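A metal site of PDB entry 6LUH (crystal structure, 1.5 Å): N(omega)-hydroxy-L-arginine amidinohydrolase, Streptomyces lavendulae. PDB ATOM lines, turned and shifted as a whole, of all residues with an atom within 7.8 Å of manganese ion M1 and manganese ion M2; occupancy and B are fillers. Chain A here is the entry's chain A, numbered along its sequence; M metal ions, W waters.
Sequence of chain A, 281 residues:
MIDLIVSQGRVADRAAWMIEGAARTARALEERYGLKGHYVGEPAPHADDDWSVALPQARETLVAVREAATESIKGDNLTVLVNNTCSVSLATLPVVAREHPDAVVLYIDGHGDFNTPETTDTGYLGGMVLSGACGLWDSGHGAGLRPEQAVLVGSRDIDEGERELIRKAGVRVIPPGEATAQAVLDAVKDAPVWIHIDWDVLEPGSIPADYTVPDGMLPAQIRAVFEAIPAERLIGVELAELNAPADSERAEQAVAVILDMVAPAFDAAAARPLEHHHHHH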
ATOM      1  N   THR A  85      20.932  -3.680  18.992  1.00  0.00           N
ATOM      2  CA  THR A  85      21.832  -2.827  19.757  1.00  0.00           C
ATOM      3  C   THR A  85      22.403  -3.582  20.958  1.00  0.00           C
ATOM      4  O   THR A  85      21.836  -4.576  21.429  1.00  0.00           O
ATOM      5  CB  THR A  85      21.110  -1.562  20.259  1.00  0.00           C
ATOM      6  OG1 THR A  85      20.092  -1.921  21.219  1.00  0.00           O
ATOM      7  CG2 THR A  85      20.470  -0.784  19.104  1.00  0.00           C
ATOM      8  N   CYS A  86      23.529  -3.093  21.452  1.00  0.00           N
ATOM      9  CA  CYS A  86      24.056  -3.630  22.703  1.00  0.00           C
ATOM     10  C   CYS A  86      23.059  -3.487  23.848  1.00  0.00           C
ATOM     11  O   CYS A  86      23.130  -4.266  24.809  1.00  0.00           O
ATOM     12  CB  CYS A  86      25.363  -2.940  23.078  1.00  0.00           C
ATOM     13  SG  CYS A  86      26.750  -3.333  22.030  1.00  0.00           S
ATOM     14  N   SER A  87      22.174  -2.488  23.779  1.00  0.00           N
ATOM     15  CA  SER A  87      21.234  -2.273  24.880  1.00  0.00           C
ATOM     16  C   SER A  87      20.303  -3.457  25.097  1.00  0.00           C
ATOM     17  O   SER A  87      19.791  -3.592  26.216  1.00  0.00           O
ATOM     18  CB  SER A  87      20.426  -0.982  24.662  1.00  0.00           C
ATOM     19  OG  SER A  87      21.302   0.126  24.576  1.00  0.00           O
ATOM     20  N   TYR A 107      33.042  -8.760  26.834  1.00  0.00           N
ATOM     21  CA  TYR A 107      32.288  -7.662  26.217  1.00  0.00           C
ATOM     22  C   TYR A 107      33.197  -7.038  25.167  1.00  0.00           C
ATOM     23  O   TYR A 107      34.068  -6.222  25.480  1.00  0.00           O
ATOM     24  CB  TYR A 107      31.838  -6.666  27.281  1.00  0.00           C
ATOM     25  CG  TYR A 107      30.696  -5.772  26.863  1.00  0.00           C
ATOM     26  CD1 TYR A 107      30.918  -4.670  26.035  1.00  0.00           C
ATOM     27  CD2 TYR A 107      29.410  -6.004  27.320  1.00  0.00           C
ATOM     28  CE1 TYR A 107      29.866  -3.839  25.645  1.00  0.00           C
ATOM     29  CE2 TYR A 107      28.356  -5.185  26.951  1.00  0.00           C
ATOM     30  CZ  TYR A 107      28.599  -4.093  26.138  1.00  0.00           C
ATOM     31  OH  TYR A 107      27.530  -3.305  25.757  1.00  0.00           O
ATOM     32  N   ILE A 108      33.015  -7.464  23.918  1.00  0.00           N
ATOM     33  CA  ILE A 108      33.928  -7.148  22.829  1.00  0.00           C
ATOM     34  C   ILE A 108      33.354  -5.952  22.078  1.00  0.00           C
ATOM     35  O   ILE A 108      32.284  -6.034  21.462  1.00  0.00           O
ATOM     36  CB  ILE A 108      34.152  -8.366  21.920  1.00  0.00           C
ATOM     37  CG1 ILE A 108      34.549  -9.593  22.753  1.00  0.00           C
ATOM     38  CG2 ILE A 108      35.222  -8.030  20.884  1.00  0.00           C
ATOM     39  CD1 ILE A 108      34.740 -10.868  21.931  1.00  0.00           C
ATOM     40  N   ASP A 109      34.047  -4.817  22.147  1.00  0.00           N
ATOM     41  CA  ASP A 109      33.428  -3.549  21.795  1.00  0.00           C
ATOM     42  C   ASP A 109      34.533  -2.527  21.656  1.00  0.00           C
ATOM     43  O   ASP A 109      35.472  -2.513  22.463  1.00  0.00           O
ATOM     44  CB  ASP A 109      32.434  -3.113  22.895  1.00  0.00           C
ATOM     45  CG  ASP A 109      31.403  -2.095  22.431  1.00  0.00           C
ATOM     46  OD1 ASP A 109      31.767  -1.124  21.721  1.00  0.00           O
ATOM     47  OD2 ASP A 109      30.241  -2.216  22.892  1.00  0.00           O
ATOM     48  N   GLY A 110      34.466  -1.696  20.622  1.00  0.00           N
ATOM     49  CA  GLY A 110      35.390  -0.573  20.543  1.00  0.00           C
ATOM     50  C   GLY A 110      35.202   0.429  21.650  1.00  0.00           C
ATOM     51  O   GLY A 110      36.135   1.188  21.968  1.00  0.00           O
ATOM     52  N   HIS A 111      34.029   0.419  22.303  1.00  0.00           N
ATOM     53  CA  HIS A 111      33.718   1.289  23.428  1.00  0.00           C
ATOM     54  C   HIS A 111      33.711   0.506  24.740  1.00  0.00           C
ATOM     55  O   HIS A 111      33.667  -0.719  24.773  1.00  0.00           O
ATOM     56  CB  HIS A 111      32.343   1.929  23.258  1.00  0.00           C
ATOM     57  CG  HIS A 111      32.201   2.751  22.024  1.00  0.00           C
ATOM     58  ND1 HIS A 111      31.760   2.225  20.836  1.00  0.00           N
ATOM     59  CD2 HIS A 111      32.410   4.074  21.813  1.00  0.00           C
ATOM     60  CE1 HIS A 111      31.698   3.183  19.929  1.00  0.00           C
ATOM     61  NE2 HIS A 111      32.070   4.319  20.499  1.00  0.00           N
ATOM     62  N   GLY A 112      33.714   1.270  25.852  1.00  0.00           N
ATOM     63  CA  GLY A 112      33.538   0.669  27.156  1.00  0.00           C
ATOM     64  C   GLY A 112      32.098   0.409  27.574  1.00  0.00           C
ATOM     65  O   GLY A 112      31.853  -0.455  28.424  1.00  0.00           O
ATOM     66  N   ASP A 113      31.135   1.147  26.986  1.00  0.00           N
ATOM     67  CA  ASP A 113      29.709   1.013  27.313  1.00  0.00           C
ATOM     68  C   ASP A 113      29.492   0.984  28.817  1.00  0.00           C
ATOM     69  O   ASP A 113      28.646   0.242  29.337  1.00  0.00           O
ATOM     70  CB  ASP A 113      29.118  -0.225  26.643  1.00  0.00           C
ATOM     71  CG  ASP A 113      28.923  -0.041  25.138  1.00  0.00           C
ATOM     72  OD1 ASP A 113      29.403   0.967  24.550  1.00  0.00           O
ATOM     73  OD2 ASP A 113      28.291  -0.931  24.561  1.00  0.00           O
ATOM     74  N   TYR A 124      22.914   8.409  25.641  1.00  0.00           N
ATOM     75  CA  TYR A 124      22.621   7.228  24.828  1.00  0.00           C
ATOM     76  C   TYR A 124      22.671   5.978  25.687  1.00  0.00           C
ATOM     77  O   TYR A 124      23.698   5.674  26.316  1.00  0.00           O
ATOM     78  CB  TYR A 124      23.598   7.153  23.664  1.00  0.00           C
ATOM     79  CG  TYR A 124      23.407   5.933  22.799  1.00  0.00           C
ATOM     80  CD1 TYR A 124      22.120   5.535  22.394  1.00  0.00           C
ATOM     81  CD2 TYR A 124      24.472   5.165  22.393  1.00  0.00           C
ATOM     82  CE1 TYR A 124      21.931   4.400  21.595  1.00  0.00           C
ATOM     83  CE2 TYR A 124      24.302   4.041  21.616  1.00  0.00           C
ATOM     84  CZ  TYR A 124      23.027   3.652  21.224  1.00  0.00           C
ATOM     85  OH  TYR A 124      22.879   2.516  20.434  1.00  0.00           O
ATOM     86  N   GLY A 126      22.876   2.946  24.817  1.00  0.00           N
ATOM     87  CA  GLY A 126      23.863   1.996  24.347  1.00  0.00           C
ATOM     88  C   GLY A 126      25.247   2.242  24.920  1.00  0.00           C
ATOM     89  O   GLY A 126      26.098   1.351  24.862  1.00  0.00           O
ATOM     90  N   GLY A 127      25.492   3.435  25.469  1.00  0.00           N
ATOM     91  CA  GLY A 127      26.741   3.708  26.157  1.00  0.00           C
ATOM     92  C   GLY A 127      26.749   3.318  27.618  1.00  0.00           C
ATOM     93  O   GLY A 127      27.744   3.557  28.300  1.00  0.00           O
ATOM     94  N   MET A 128      25.668   2.686  28.096  1.00  0.00           N
ATOM     95  CA  MET A 128      25.428   2.446  29.520  1.00  0.00           C
ATOM     96  C   MET A 128      25.128   0.979  29.814  1.00  0.00           C
ATOM     97  O   MET A 128      24.635   0.659  30.901  1.00  0.00           O
ATOM     98  CB  MET A 128      24.249   3.306  30.003  1.00  0.00           C
ATOM     99  CG  MET A 128      24.408   4.811  29.709  1.00  0.00           C
ATOM    100  SD  MET A 128      22.852   5.776  29.707  1.00  0.00           S
ATOM    101  CE  MET A 128      22.381   5.639  31.430  1.00  0.00           C
ATOM    102  N   VAL A 129      25.434   0.074  28.868  1.00  0.00           N
ATOM    103  CA  VAL A 129      24.956  -1.298  28.967  1.00  0.00           C
ATOM    104  C   VAL A 129      25.733  -2.079  30.020  1.00  0.00           C
ATOM    105  O   VAL A 129      25.156  -2.756  30.870  1.00  0.00           O
ATOM    106  CB  VAL A 129      25.053  -1.993  27.593  1.00  0.00           C
ATOM    107  CG1 VAL A 129      24.587  -3.449  27.697  1.00  0.00           C
ATOM    108  CG2 VAL A 129      24.262  -1.232  26.534  1.00  0.00           C
ATOM    109  N   LEU A 130      27.061  -2.046  29.944  1.00  0.00           N
ATOM    110  CA  LEU A 130      27.828  -2.914  30.824  1.00  0.00           C
ATOM    111  C   LEU A 130      27.775  -2.406  32.260  1.00  0.00           C
ATOM    112  O   LEU A 130      27.698  -3.208  33.204  1.00  0.00           O
ATOM    113  CB  LEU A 130      29.261  -3.062  30.301  1.00  0.00           C
ATOM    114  CG  LEU A 130      30.201  -3.968  31.097  1.00  0.00           C
ATOM    115  CD1 LEU A 130      29.619  -5.370  31.230  1.00  0.00           C
ATOM    116  CD2 LEU A 130      31.566  -4.003  30.459  1.00  0.00           C
ATOM    117  N   SER A 155      38.396  -2.557  23.389  1.00  0.00           N
ATOM    118  CA  SER A 155      38.029  -1.177  23.654  1.00  0.00           C
ATOM    119  C   SER A 155      39.266  -0.280  23.654  1.00  0.00           C
ATOM    120  O   SER A 155      40.352  -0.679  24.099  1.00  0.00           O
ATOM    121  CB  SER A 155      37.322  -1.081  25.016  1.00  0.00           C
ATOM    122  OG  SER A 155      36.425  -2.164  25.277  1.00  0.00           O
ATOM    123  N   HIS A 196      29.793 -11.221  24.134  1.00  0.00           N
ATOM    124  CA  HIS A 196      28.965 -10.133  23.616  1.00  0.00           C
ATOM    125  C   HIS A 196      29.803  -9.316  22.624  1.00  0.00           C
ATOM    126  O   HIS A 196      30.865  -8.813  22.995  1.00  0.00           O
ATOM    127  CB  HIS A 196      28.461  -9.262  24.763  1.00  0.00           C
ATOM    128  CG  HIS A 196      27.824  -7.963  24.351  1.00  0.00           C
ATOM    129  ND1 HIS A 196      26.468  -7.749  24.419  1.00  0.00           N
ATOM    130  CD2 HIS A 196      28.365  -6.813  23.863  1.00  0.00           C
ATOM    131  CE1 HIS A 196      26.190  -6.520  24.008  1.00  0.00           C
ATOM    132  NE2 HIS A 196      27.324  -5.942  23.640  1.00  0.00           N
ATOM    133  N   ILE A 197      29.338  -9.166  21.382  1.00  0.00           N
ATOM    134  CA  ILE A 197      30.137  -8.472  20.375  1.00  0.00           C
ATOM    135  C   ILE A 197      29.370  -7.274  19.830  1.00  0.00           C
ATOM    136  O   ILE A 197      28.251  -7.430  19.324  1.00  0.00           O
ATOM    137  CB  ILE A 197      30.560  -9.387  19.221  1.00  0.00           C
ATOM    138  CG1 ILE A 197      31.442 -10.515  19.729  1.00  0.00           C
ATOM    139  CG2 ILE A 197      31.295  -8.572  18.162  1.00  0.00           C
ATOM    140  CD1 ILE A 197      31.726 -11.575  18.685  1.00  0.00           C
ATOM    141  N   ASP A 198      29.993  -6.096  19.910  1.00  0.00           N
ATOM    142  CA  ASP A 198      29.582  -4.891  19.198  1.00  0.00           C
ATOM    143  C   ASP A 198      30.526  -4.724  18.005  1.00  0.00           C
ATOM    144  O   ASP A 198      31.727  -4.571  18.188  1.00  0.00           O
ATOM    145  CB  ASP A 198      29.630  -3.716  20.168  1.00  0.00           C
ATOM    146  CG  ASP A 198      29.371  -2.344  19.536  1.00  0.00           C
ATOM    147  OD1 ASP A 198      29.371  -2.209  18.274  1.00  0.00           O
ATOM    148  OD2 ASP A 198      29.241  -1.378  20.342  1.00  0.00           O
ATOM    149  N   TRP A 199      29.978  -4.764  16.794  1.00  0.00           N
ATOM    150  CA  TRP A 199      30.854  -4.814  15.618  1.00  0.00           C
ATOM    151  C   TRP A 199      31.694  -3.564  15.402  1.00  0.00           C
ATOM    152  O   TRP A 199      32.637  -3.620  14.597  1.00  0.00           O
ATOM    153  CB  TRP A 199      30.033  -5.094  14.355  1.00  0.00           C
ATOM    154  CG  TRP A 199      29.405  -6.472  14.358  1.00  0.00           C
ATOM    155  CD1 TRP A 199      28.077  -6.761  14.201  1.00  0.00           C
ATOM    156  CD2 TRP A 199      30.067  -7.744  14.507  1.00  0.00           C
ATOM    157  NE1 TRP A 199      27.871  -8.103  14.264  1.00  0.00           N
ATOM    158  CE2 TRP A 199      29.071  -8.732  14.463  1.00  0.00           C
ATOM    159  CE3 TRP A 199      31.398  -8.122  14.703  1.00  0.00           C
ATOM    160  CZ2 TRP A 199      29.361 -10.102  14.585  1.00  0.00           C
ATOM    161  CZ3 TRP A 199      31.678  -9.473  14.838  1.00  0.00           C
ATOM    162  CH2 TRP A 199      30.667 -10.447  14.785  1.00  0.00           C
ATOM    163  N   ASP A 200      31.416  -2.457  16.118  1.00  0.00           N
ATOM    164  CA  ASP A 200      32.327  -1.323  15.974  1.00  0.00           C
ATOM    165  C   ASP A 200      33.674  -1.580  16.617  1.00  0.00           C
ATOM    166  O   ASP A 200      34.558  -0.729  16.531  1.00  0.00           O
ATOM    167  CB  ASP A 200      31.717   0.002  16.490  1.00  0.00           C
ATOM    168  CG  ASP A 200      31.388   0.004  17.989  1.00  0.00           C
ATOM    169  OD1 ASP A 200      32.108  -0.669  18.765  1.00  0.00           O
ATOM    170  OD2 ASP A 200      30.436   0.752  18.393  1.00  0.00           O
ATOM    171  N   VAL A 201      33.847  -2.762  17.207  1.00  0.00           N
ATOM    172  CA  VAL A 201      35.187  -3.186  17.646  1.00  0.00           C
ATOM    173  C   VAL A 201      36.113  -3.405  16.432  1.00  0.00           C
ATOM    174  O   VAL A 201      37.343  -3.308  16.562  1.00  0.00           O
ATOM    175  CB  VAL A 201      35.073  -4.444  18.508  1.00  0.00           C
ATOM    176  CG1 VAL A 201      34.895  -5.704  17.639  1.00  0.00           C
ATOM    177  CG2 VAL A 201      36.309  -4.583  19.410  1.00  0.00           C
ATOM    178  N   ALA A 240      25.852  -7.980  17.952  1.00  0.00           N
ATOM    179  CA  ALA A 240      25.123  -6.717  18.021  1.00  0.00           C
ATOM    180  C   ALA A 240      25.745  -5.632  17.142  1.00  0.00           C
ATOM    181  O   ALA A 240      26.963  -5.601  16.921  1.00  0.00           O
ATOM    182  CB  ALA A 240      25.033  -6.218  19.450  1.00  0.00           C
ATOM    183  N   GLU A 241      24.873  -4.746  16.669  1.00  0.00           N
ATOM    184  CA  GLU A 241      25.230  -3.478  16.034  1.00  0.00           C
ATOM    185  C   GLU A 241      25.921  -3.662  14.676  1.00  0.00           C
ATOM    186  O   GLU A 241      26.969  -3.090  14.398  1.00  0.00           O
ATOM    187  CB  GLU A 241      26.066  -2.611  16.987  1.00  0.00           C
ATOM    188  CG  GLU A 241      25.344  -2.488  18.347  1.00  0.00           C
ATOM    189  CD  GLU A 241      25.411  -1.109  19.008  1.00  0.00           C
ATOM    190  OE1 GLU A 241      26.082  -0.189  18.473  1.00  0.00           O
ATOM    191  OE2 GLU A 241      24.770  -0.942  20.078  1.00  0.00           O
HETATM  192 MN    MN M   1      30.740   0.184  20.532  1.00  0.00          MN
HETATM  193 MN    MN M   2      28.295  -1.375  22.326  1.00  0.00          MN
HETATM  194  O   HOH W   1      26.581  -0.010  21.963  1.00  0.00           O
HETATM  195  O   HOH W   2      29.290   0.741  21.959  1.00  0.00           O
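Of the 25 residues printed, 4 come within 4 Å of manganese ion M2.
N of Asp 198 is in hydrogen-bond range of O of Ile 108, 2.8 Å away.
OD1 of Asp 200 sits close to N of Gly 110 (3.2 Å).
OD2 of Asp 113 sits close to OH of Tyr 107 (2.8 Å).
N of Val 129 is in hydrogen-bond range of O of Asp 113 (3.3 Å).
The backbone carbonyl oxygen (O) of Asp 113 lies within hydrogen-bond range of the backbone NH (N) of Leu 130.
O of His 111 lies within hydrogen-bond range of OG of Ser 155 (3.2 Å).
The backbone NH (N) of Cys 86 lies within hydrogen-bond range of the side-chain carboxylate (OE2) of Glu 241, at 2.8 Å.
The side-chain sulfur of Cys 86 sits close to a ring nitrogen (NE2) of His 196, at 3.1 Å.
Four residues have an atom within 4 Å of manganese ion M1: Asp 109, His 111, Asp 198 and Asp 200.
The nearest printed residue that does not touch manganese ion M1 is Gly 110 (4.2 Å).
Water W1 bridges the side-chain carboxylate of Glu 241 (2.8 Å) and the backbone carbonyl oxygen of Gly 126 (3.2 Å).
OD1 of Asp 109 is bound to manganese ion M1.
Water W2 is bound to manganese ion M1 (2.1 Å).
Manganese ion M1 is bound by OD2 of Asp 198 (2.2 Å).
OD2 of Asp 200 is bound to manganese ion M1.
ND1 of His 111 is bound to manganese ion M1 (2.3 Å).
OD1 of Asp 200 is bound to manganese ion M1 (2.4 Å).
Manganese ion M2 is bound by OD2 of Asp 109.
OD2 of Asp 198 binds manganese ion M2.
Water W1 binds manganese ion M2 (2.2 Å).
OD2 of Asp 113 binds manganese ion M2 (2.3 Å).
Manganese ion M2 is bound by water W2 (2.4 Å).
SG of Cys 86 is bound to manganese ion M2 (2.5 Å).
Manganese ion M2 has six donor atoms within binding distance.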
